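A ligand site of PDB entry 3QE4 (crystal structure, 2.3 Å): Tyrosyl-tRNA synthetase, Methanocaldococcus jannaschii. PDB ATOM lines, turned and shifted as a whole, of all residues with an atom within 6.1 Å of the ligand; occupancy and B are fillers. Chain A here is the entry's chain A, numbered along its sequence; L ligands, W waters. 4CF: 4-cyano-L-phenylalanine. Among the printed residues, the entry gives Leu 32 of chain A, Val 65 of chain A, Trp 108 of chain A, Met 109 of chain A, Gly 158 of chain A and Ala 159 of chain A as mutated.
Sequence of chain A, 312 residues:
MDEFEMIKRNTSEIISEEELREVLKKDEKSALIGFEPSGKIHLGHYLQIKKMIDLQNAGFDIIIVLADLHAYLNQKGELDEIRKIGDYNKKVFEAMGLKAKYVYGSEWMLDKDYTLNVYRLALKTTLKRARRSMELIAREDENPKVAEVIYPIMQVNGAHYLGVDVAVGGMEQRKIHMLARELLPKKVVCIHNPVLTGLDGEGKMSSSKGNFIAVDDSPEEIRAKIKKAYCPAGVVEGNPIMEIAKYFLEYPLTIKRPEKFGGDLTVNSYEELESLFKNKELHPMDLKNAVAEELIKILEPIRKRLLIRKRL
OE1 of Gln 155 is in hydrogen-bond range of N of the ligand, 2.4 Å away.
The side-chain amide nitrogen of Gln 173 is in hydrogen-bond range of an oxygen (O) of the ligand (2.6 Å).
The side-chain hydroxyl of Tyr 151 sits at hydrogen-bond distance from a nitrogen (N) of the ligand (2.7 Å).
O of Gly 34 lies close to OXT of the ligand.
The side-chain amide nitrogen (NE2) of Gln 173 is in hydrogen-bond range of the side-chain carboxylate (OE2) of Glu 172 (3.1 Å).
The backbone NH of Gly 158 lies within hydrogen-bond range of the side-chain hydroxyl of Tyr 114 (3.2 Å).
N of Phe 35 lies within hydrogen-bond range of O of Val 65 (2.9 Å).
OH of Tyr 151 is in hydrogen-bond range of OE2 of Glu 36 (2.6 Å).
NE2 of Gln 155 is in hydrogen-bond range of OE1 of Gln 173, at 3.1 Å.
The backbone carbonyl oxygen (O) of Phe 35 sits at hydrogen-bond distance from the backbone NH (N) of Ala 67 (2.9 Å).
Merely in contact with the ligand: Leu 32, Phe 35, Glu 36, Ala 67, His 70, Trp 108, Met 109, Gly 158 and Ala 159.
Hydrophobic or aromatic side chains within 4 Å of the ligand: Leu 32, Ala 67, His 70, Trp 108, Met 109 and Tyr 151.
13 residues have an atom within 4 Å of the ligand: Leu 32, Gly 34, Phe 35, Glu 36, Ala 67, His 70, Trp 108, Met 109, Tyr 151, Gln 155, Gly 158, Ala 159 and Gln 173.
Water W1 lies within hydrogen-bond range of the backbone carbonyl oxygen (O) of Gly 34 and an oxygen (OXT) of the ligand.
Water W3 lies within hydrogen-bond range of OXT of the ligand (2.8 Å) and N of Glu 36 (2.9 Å).
Water W2 lies within hydrogen-bond range of OE2 of Glu 36 (2.7 Å) and O of the ligand (3.2 Å).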
ATOM      1  N   LEU A  32     -17.768  27.900  -2.984  1.00  0.00           N
ATOM      2  CA  LEU A  32     -18.554  27.094  -2.084  1.00  0.00           C
ATOM      3  C   LEU A  32     -19.067  25.848  -2.765  1.00  0.00           C
ATOM      4  O   LEU A  32     -19.208  25.762  -3.982  1.00  0.00           O
ATOM      5  CB  LEU A  32     -19.731  27.858  -1.411  1.00  0.00           C
ATOM      6  CG  LEU A  32     -20.986  28.271  -2.270  1.00  0.00           C
ATOM      7  CD1 LEU A  32     -21.859  27.089  -2.685  1.00  0.00           C
ATOM      8  CD2 LEU A  32     -21.887  29.182  -1.499  1.00  0.00           C
ATOM      9  N   ILE A  33     -19.381  24.900  -1.910  1.00  0.00           N
ATOM     10  CA  ILE A  33     -20.093  23.691  -2.171  1.00  0.00           C
ATOM     11  C   ILE A  33     -20.904  23.489  -0.914  1.00  0.00           C
ATOM     12  O   ILE A  33     -20.442  23.770   0.187  1.00  0.00           O
ATOM     13  CB  ILE A  33     -19.189  22.502  -2.512  1.00  0.00           C
ATOM     14  CG1 ILE A  33     -20.028  21.313  -3.099  1.00  0.00           C
ATOM     15  CG2 ILE A  33     -18.298  22.097  -1.319  1.00  0.00           C
ATOM     16  CD1 ILE A  33     -19.179  20.243  -3.728  1.00  0.00           C
ATOM     17  N   GLY A  34     -22.097  22.993  -1.082  1.00  0.00           N
ATOM     18  CA  GLY A  34     -22.951  22.665   0.037  1.00  0.00           C
ATOM     19  C   GLY A  34     -23.422  21.244  -0.100  1.00  0.00           C
ATOM     20  O   GLY A  34     -23.506  20.729  -1.216  1.00  0.00           O
ATOM     21  N   PHE A  35     -23.692  20.590   1.030  1.00  0.00           N
ATOM     22  CA  PHE A  35     -24.202  19.219   1.095  1.00  0.00           C
ATOM     23  C   PHE A  35     -25.278  19.103   2.134  1.00  0.00           C
ATOM     24  O   PHE A  35     -25.096  19.567   3.255  1.00  0.00           O
ATOM     25  CB  PHE A  35     -23.101  18.212   1.480  1.00  0.00           C
ATOM     26  CG  PHE A  35     -21.833  18.140   0.651  1.00  0.00           C
ATOM     27  CD1 PHE A  35     -21.797  17.390  -0.519  1.00  0.00           C
ATOM     28  CD2 PHE A  35     -20.655  18.718   1.108  1.00  0.00           C
ATOM     29  CE1 PHE A  35     -20.600  17.243  -1.236  1.00  0.00           C
ATOM     30  CE2 PHE A  35     -19.459  18.552   0.404  1.00  0.00           C
ATOM     31  CZ  PHE A  35     -19.445  17.818  -0.760  1.00  0.00           C
ATOM     32  N   GLU A  36     -26.373  18.431   1.790  1.00  0.00           N
ATOM     33  CA  GLU A  36     -27.437  18.162   2.742  1.00  0.00           C
ATOM     34  C   GLU A  36     -26.796  17.109   3.689  1.00  0.00           C
ATOM     35  O   GLU A  36     -26.279  16.140   3.184  1.00  0.00           O
ATOM     36  CB  GLU A  36     -28.628  17.504   2.027  1.00  0.00           C
ATOM     37  CG  GLU A  36     -29.681  18.439   1.433  1.00  0.00           C
ATOM     38  CD  GLU A  36     -30.862  17.675   0.849  1.00  0.00           C
ATOM     39  OE1 GLU A  36     -31.412  16.776   1.534  1.00  0.00           O
ATOM     40  OE2 GLU A  36     -31.237  17.964  -0.311  1.00  0.00           O
ATOM     41  N   VAL A  65     -20.843  24.390   2.974  1.00  0.00           N
ATOM     42  CA  VAL A  65     -22.114  24.613   3.637  1.00  0.00           C
ATOM     43  C   VAL A  65     -22.698  23.269   4.054  1.00  0.00           C
ATOM     44  O   VAL A  65     -22.986  22.399   3.204  1.00  0.00           O
ATOM     45  CB  VAL A  65     -23.114  25.455   2.803  1.00  0.00           C
ATOM     46  CG1 VAL A  65     -24.317  25.863   3.644  1.00  0.00           C
ATOM     47  CG2 VAL A  65     -22.443  26.690   2.188  1.00  0.00           C
ATOM     48  N   ALA A  67     -25.735  21.942   4.852  1.00  0.00           N
ATOM     49  CA  ALA A  67     -27.098  22.414   4.585  1.00  0.00           C
ATOM     50  C   ALA A  67     -28.182  21.667   5.351  1.00  0.00           C
ATOM     51  O   ALA A  67     -29.025  20.962   4.754  1.00  0.00           O
ATOM     52  CB  ALA A  67     -27.378  22.440   3.087  1.00  0.00           C
ATOM     53  N   HIS A  70     -31.821  22.756   4.405  1.00  0.00           N
ATOM     54  CA  HIS A  70     -32.223  22.211   3.118  1.00  0.00           C
ATOM     55  C   HIS A  70     -32.657  20.760   3.223  1.00  0.00           C
ATOM     56  O   HIS A  70     -33.669  20.384   2.613  1.00  0.00           O
ATOM     57  CB  HIS A  70     -31.090  22.344   2.124  1.00  0.00           C
ATOM     58  CG  HIS A  70     -31.024  23.709   1.544  1.00  0.00           C
ATOM     59  ND1 HIS A  70     -31.754  24.049   0.405  1.00  0.00           N
ATOM     60  CD2 HIS A  70     -30.334  24.791   1.973  1.00  0.00           C
ATOM     61  CE1 HIS A  70     -31.492  25.327   0.202  1.00  0.00           C
ATOM     62  NE2 HIS A  70     -30.633  25.819   1.121  1.00  0.00           N
ATOM     63  N   TRP A 108     -26.823  31.175   9.480  1.00  0.00           N
ATOM     64  CA  TRP A 108     -27.123  32.346   8.646  1.00  0.00           C
ATOM     65  C   TRP A 108     -28.345  32.279   7.719  1.00  0.00           C
ATOM     66  O   TRP A 108     -28.771  33.329   7.233  1.00  0.00           O
ATOM     67  CB  TRP A 108     -25.868  32.766   7.864  1.00  0.00           C
ATOM     68  CG  TRP A 108     -25.257  31.631   7.097  1.00  0.00           C
ATOM     69  CD1 TRP A 108     -24.458  30.642   7.600  1.00  0.00           C
ATOM     70  CD2 TRP A 108     -25.408  31.350   5.710  1.00  0.00           C
ATOM     71  NE1 TRP A 108     -24.129  29.745   6.612  1.00  0.00           N
ATOM     72  CE2 TRP A 108     -24.663  30.178   5.427  1.00  0.00           C
ATOM     73  CE3 TRP A 108     -26.060  32.001   4.646  1.00  0.00           C
ATOM     74  CZ2 TRP A 108     -24.572  29.632   4.140  1.00  0.00           C
ATOM     75  CZ3 TRP A 108     -25.973  31.459   3.373  1.00  0.00           C
ATOM     76  CH2 TRP A 108     -25.245  30.284   3.132  1.00  0.00           C
ATOM     77  N   MET A 109     -28.931  31.093   7.479  1.00  0.00           N
ATOM     78  CA  MET A 109     -30.098  31.070   6.580  1.00  0.00           C
ATOM     79  C   MET A 109     -31.414  31.527   7.247  1.00  0.00           C
ATOM     80  O   MET A 109     -32.458  31.508   6.592  1.00  0.00           O
ATOM     81  CB  MET A 109     -30.246  29.738   5.838  1.00  0.00           C
ATOM     82  CG  MET A 109     -29.073  29.427   4.954  1.00  0.00           C
ATOM     83  SD  MET A 109     -29.269  27.851   4.100  1.00  0.00           S
ATOM     84  CE  MET A 109     -27.653  27.697   3.385  1.00  0.00           C
ATOM     85  N   TYR A 114     -31.081  37.690   5.290  1.00  0.00           N
ATOM     86  CA  TYR A 114     -31.129  36.508   4.449  1.00  0.00           C
ATOM     87  C   TYR A 114     -32.579  36.235   4.024  1.00  0.00           C
ATOM     88  O   TYR A 114     -32.922  36.361   2.851  1.00  0.00           O
ATOM     89  CB  TYR A 114     -30.532  35.291   5.187  1.00  0.00           C
ATOM     90  CG  TYR A 114     -30.288  34.125   4.269  1.00  0.00           C
ATOM     91  CD1 TYR A 114     -29.051  33.956   3.635  1.00  0.00           C
ATOM     92  CD2 TYR A 114     -31.314  33.233   3.937  1.00  0.00           C
ATOM     93  CE1 TYR A 114     -28.841  32.926   2.721  1.00  0.00           C
ATOM     94  CE2 TYR A 114     -31.108  32.189   3.049  1.00  0.00           C
ATOM     95  CZ  TYR A 114     -29.864  32.034   2.443  1.00  0.00           C
ATOM     96  OH  TYR A 114     -29.630  31.033   1.548  1.00  0.00           O
ATOM     97  N   ILE A 137     -33.620  16.427  -7.225  1.00  0.00           N
ATOM     98  CA  ILE A 137     -33.200  16.644  -5.860  1.00  0.00           C
ATOM     99  C   ILE A 137     -34.209  16.194  -4.842  1.00  0.00           C
ATOM    100  O   ILE A 137     -33.828  15.577  -3.832  1.00  0.00           O
ATOM    101  CB  ILE A 137     -32.649  18.079  -5.648  1.00  0.00           C
ATOM    102  CG1 ILE A 137     -31.417  18.299  -6.602  1.00  0.00           C
ATOM    103  CG2 ILE A 137     -32.300  18.395  -4.131  1.00  0.00           C
ATOM    104  CD1 ILE A 137     -30.725  19.657  -6.647  1.00  0.00           C
ATOM    105  N   TYR A 151     -36.712  25.515  -1.011  1.00  0.00           N
ATOM    106  CA  TYR A 151     -35.407  24.865  -1.155  1.00  0.00           C
ATOM    107  C   TYR A 151     -34.545  25.486  -2.292  1.00  0.00           C
ATOM    108  O   TYR A 151     -33.484  25.985  -1.950  1.00  0.00           O
ATOM    109  CB  TYR A 151     -35.575  23.334  -1.323  1.00  0.00           C
ATOM    110  CG  TYR A 151     -34.293  22.523  -1.387  1.00  0.00           C
ATOM    111  CD1 TYR A 151     -34.049  21.490  -0.493  1.00  0.00           C
ATOM    112  CD2 TYR A 151     -33.342  22.757  -2.375  1.00  0.00           C
ATOM    113  CE1 TYR A 151     -32.893  20.705  -0.569  1.00  0.00           C
ATOM    114  CE2 TYR A 151     -32.166  22.001  -2.456  1.00  0.00           C
ATOM    115  CZ  TYR A 151     -31.934  20.988  -1.525  1.00  0.00           C
ATOM    116  OH  TYR A 151     -30.794  20.202  -1.589  1.00  0.00           O
ATOM    117  N   MET A 154     -33.429  29.251  -1.508  1.00  0.00           N
ATOM    118  CA  MET A 154     -32.560  29.379  -0.358  1.00  0.00           C
ATOM    119  C   MET A 154     -31.160  28.958  -0.746  1.00  0.00           C
ATOM    120  O   MET A 154     -30.187  29.476  -0.202  1.00  0.00           O
ATOM    121  CB  MET A 154     -33.071  28.499   0.758  1.00  0.00           C
ATOM    122  CG  MET A 154     -34.320  29.044   1.375  1.00  0.00           C
ATOM    123  SD  MET A 154     -34.576  28.512   3.082  1.00  0.00           S
ATOM    124  CE  MET A 154     -33.267  27.230   3.307  1.00  0.00           C
ATOM    125  N   GLN A 155     -31.064  28.000  -1.683  1.00  0.00           N
ATOM    126  CA  GLN A 155     -29.774  27.532  -2.171  1.00  0.00           C
ATOM    127  C   GLN A 155     -29.148  28.660  -2.990  1.00  0.00           C
ATOM    128  O   GLN A 155     -28.030  29.071  -2.700  1.00  0.00           O
ATOM    129  CB  GLN A 155     -29.935  26.245  -2.991  1.00  0.00           C
ATOM    130  CG  GLN A 155     -28.587  25.715  -3.493  1.00  0.00           C
ATOM    131  CD  GLN A 155     -28.671  24.316  -4.029  1.00  0.00           C
ATOM    132  OE1 GLN A 155     -29.457  23.492  -3.561  1.00  0.00           O
ATOM    133  NE2 GLN A 155     -27.798  24.000  -4.976  1.00  0.00           N
ATOM    134  N   VAL A 156     -29.945  29.229  -3.940  1.00  0.00           N
ATOM    135  CA  VAL A 156     -29.585  30.360  -4.809  1.00  0.00           C
ATOM    136  C   VAL A 156     -29.032  31.533  -3.970  1.00  0.00           C
ATOM    137  O   VAL A 156     -27.982  32.070  -4.296  1.00  0.00           O
ATOM    138  CB  VAL A 156     -30.814  30.735  -5.704  1.00  0.00           C
ATOM    139  CG1 VAL A 156     -30.675  32.116  -6.318  1.00  0.00           C
ATOM    140  CG2 VAL A 156     -31.069  29.690  -6.781  1.00  0.00           C
ATOM    141  N   ASN A 157     -29.690  31.876  -2.873  1.00  0.00           N
ATOM    142  CA  ASN A 157     -29.330  32.989  -1.997  1.00  0.00           C
ATOM    143  C   ASN A 157     -28.064  32.770  -1.148  1.00  0.00           C
ATOM    144  O   ASN A 157     -27.457  33.755  -0.708  1.00  0.00           O
ATOM    145  CB  ASN A 157     -30.525  33.406  -1.112  1.00  0.00           C
ATOM    146  CG  ASN A 157     -30.388  34.749  -0.480  1.00  0.00           C
ATOM    147  OD1 ASN A 157     -29.964  35.718  -1.121  1.00  0.00           O
ATOM    148  ND2 ASN A 157     -30.800  34.861   0.777  1.00  0.00           N
ATOM    149  N   GLY A 158     -27.682  31.517  -0.942  1.00  0.00           N
ATOM    150  CA  GLY A 158     -26.479  31.178  -0.192  1.00  0.00           C
ATOM    151  C   GLY A 158     -25.236  31.650  -0.917  1.00  0.00           C
ATOM    152  O   GLY A 158     -24.325  32.188  -0.287  1.00  0.00           O
ATOM    153  N   ALA A 159     -25.235  31.511  -2.269  1.00  0.00           N
ATOM    154  CA  ALA A 159     -24.151  31.938  -3.157  1.00  0.00           C
ATOM    155  C   ALA A 159     -24.014  33.442  -3.116  1.00  0.00           C
ATOM    156  O   ALA A 159     -22.890  33.952  -3.199  1.00  0.00           O
ATOM    157  CB  ALA A 159     -24.438  31.477  -4.580  1.00  0.00           C
ATOM    158  N   LEU A 162     -22.967  34.615   0.774  1.00  0.00           N
ATOM    159  CA  LEU A 162     -21.566  34.324   0.965  1.00  0.00           C
ATOM    160  C   LEU A 162     -20.616  35.085   0.076  1.00  0.00           C
ATOM    161  O   LEU A 162     -19.437  35.181   0.406  1.00  0.00           O
ATOM    162  CB  LEU A 162     -21.311  32.819   0.940  1.00  0.00           C
ATOM    163  CG  LEU A 162     -21.947  32.028   2.086  1.00  0.00           C
ATOM    164  CD1 LEU A 162     -21.841  30.544   1.819  1.00  0.00           C
ATOM    165  CD2 LEU A 162     -21.320  32.397   3.428  1.00  0.00           C
ATOM    166  N   GLU A 172     -26.593  17.071 -11.002  1.00  0.00           N
ATOM    167  CA  GLU A 172     -27.999  17.196 -10.610  1.00  0.00           C
ATOM    168  C   GLU A 172     -28.374  18.602 -10.061  1.00  0.00           C
ATOM    169  O   GLU A 172     -29.560  18.896  -9.989  1.00  0.00           O
ATOM    170  CB  GLU A 172     -28.399  16.081  -9.626  1.00  0.00           C
ATOM    171  CG  GLU A 172     -27.815  16.230  -8.220  1.00  0.00           C
ATOM    172  CD  GLU A 172     -26.318  16.041  -8.038  1.00  0.00           C
ATOM    173  OE1 GLU A 172     -25.729  15.185  -8.765  1.00  0.00           O
ATOM    174  OE2 GLU A 172     -25.747  16.707  -7.143  1.00  0.00           O
ATOM    175  N   GLN A 173     -27.370  19.441  -9.666  1.00  0.00           N
ATOM    176  CA  GLN A 173     -27.517  20.809  -9.155  1.00  0.00           C
ATOM    177  C   GLN A 173     -27.611  21.851 -10.299  1.00  0.00           C
ATOM    178  O   GLN A 173     -27.815  23.058 -10.031  1.00  0.00           O
ATOM    179  CB  GLN A 173     -26.309  21.213  -8.286  1.00  0.00           C
ATOM    180  CG  GLN A 173     -25.938  20.238  -7.187  1.00  0.00           C
ATOM    181  CD  GLN A 173     -26.952  20.127  -6.083  1.00  0.00           C
ATOM    182  OE1 GLN A 173     -27.728  21.045  -5.807  1.00  0.00           O
ATOM    183  NE2 GLN A 173     -26.941  18.999  -5.406  1.00  0.00           N
ATOM    184  N   ILE A 176     -30.683  24.389 -10.386  1.00  0.00           N
ATOM    185  CA  ILE A 176     -30.636  25.382  -9.323  1.00  0.00           C
ATOM    186  C   ILE A 176     -29.512  26.408  -9.606  1.00  0.00           C
ATOM    187  O   ILE A 176     -29.695  27.608  -9.377  1.00  0.00           O
ATOM    188  CB  ILE A 176     -30.520  24.708  -7.923  1.00  0.00           C
ATOM    189  CG1 ILE A 176     -31.757  23.795  -7.676  1.00  0.00           C
ATOM    190  CG2 ILE A 176     -30.356  25.763  -6.816  1.00  0.00           C
ATOM    191  CD1 ILE A 176     -31.806  23.027  -6.321  1.00  0.00           C
ATOM    192  N   HIS A 177     -28.383  25.928 -10.140  1.00  0.00           N
ATOM    193  CA  HIS A 177     -27.235  26.769 -10.513  1.00  0.00           C
ATOM    194  C   HIS A 177     -27.569  27.712 -11.701  1.00  0.00           C
ATOM    195  O   HIS A 177     -27.107  28.858 -11.709  1.00  0.00           O
ATOM    196  CB  HIS A 177     -25.992  25.882 -10.736  1.00  0.00           C
ATOM    197  CG  HIS A 177     -25.339  25.456  -9.445  1.00  0.00           C
ATOM    198  ND1 HIS A 177     -24.299  24.525  -9.427  1.00  0.00           N
ATOM    199  CD2 HIS A 177     -25.596  25.831  -8.166  1.00  0.00           C
ATOM    200  CE1 HIS A 177     -23.967  24.387  -8.155  1.00  0.00           C
ATOM    201  NE2 HIS A 177     -24.722  25.147  -7.361  1.00  0.00           N
HETATM  202  C   4CF L   1     -26.955  19.628  -2.426  1.00  0.00           C
HETATM  203  N   4CF L   1     -28.752  21.227  -3.113  1.00  0.00           N
HETATM  204  O   4CF L   1     -27.749  18.732  -2.917  1.00  0.00           O
HETATM  205  C1  4CF L   1     -25.786  27.307  -0.361  1.00  0.00           C
HETATM  206  N1  4CF L   1     -25.452  28.411  -0.196  1.00  0.00           N
HETATM  207  CA  4CF L   1     -27.470  21.066  -2.369  1.00  0.00           C
HETATM  208  CB  4CF L   1     -27.463  21.648  -0.966  1.00  0.00           C
HETATM  209  CG  4CF L   1     -27.036  23.089  -0.851  1.00  0.00           C
HETATM  210  CZ  4CF L   1     -26.159  25.850  -0.573  1.00  0.00           C
HETATM  211  CD1 4CF L   1     -25.903  23.644  -1.692  1.00  0.00           C
HETATM  212  CD2 4CF L   1     -27.668  23.874   0.091  1.00  0.00           C
HETATM  213  CE1 4CF L   1     -25.516  25.058  -1.517  1.00  0.00           C
HETATM  214  CE2 4CF L   1     -27.229  25.250   0.295  1.00  0.00           C
HETATM  215  OXT 4CF L   1     -25.778  19.349  -2.030  1.00  0.00           O
HETATM  216  O   HOH W   1     -23.305  18.721  -2.925  1.00  0.00           O
HETATM  217  O   HOH W   2     -29.742  16.410  -2.006  1.00  0.00           O
HETATM  218  O   HOH W   3     -26.671  17.016  -0.692  1.00  0.00           O
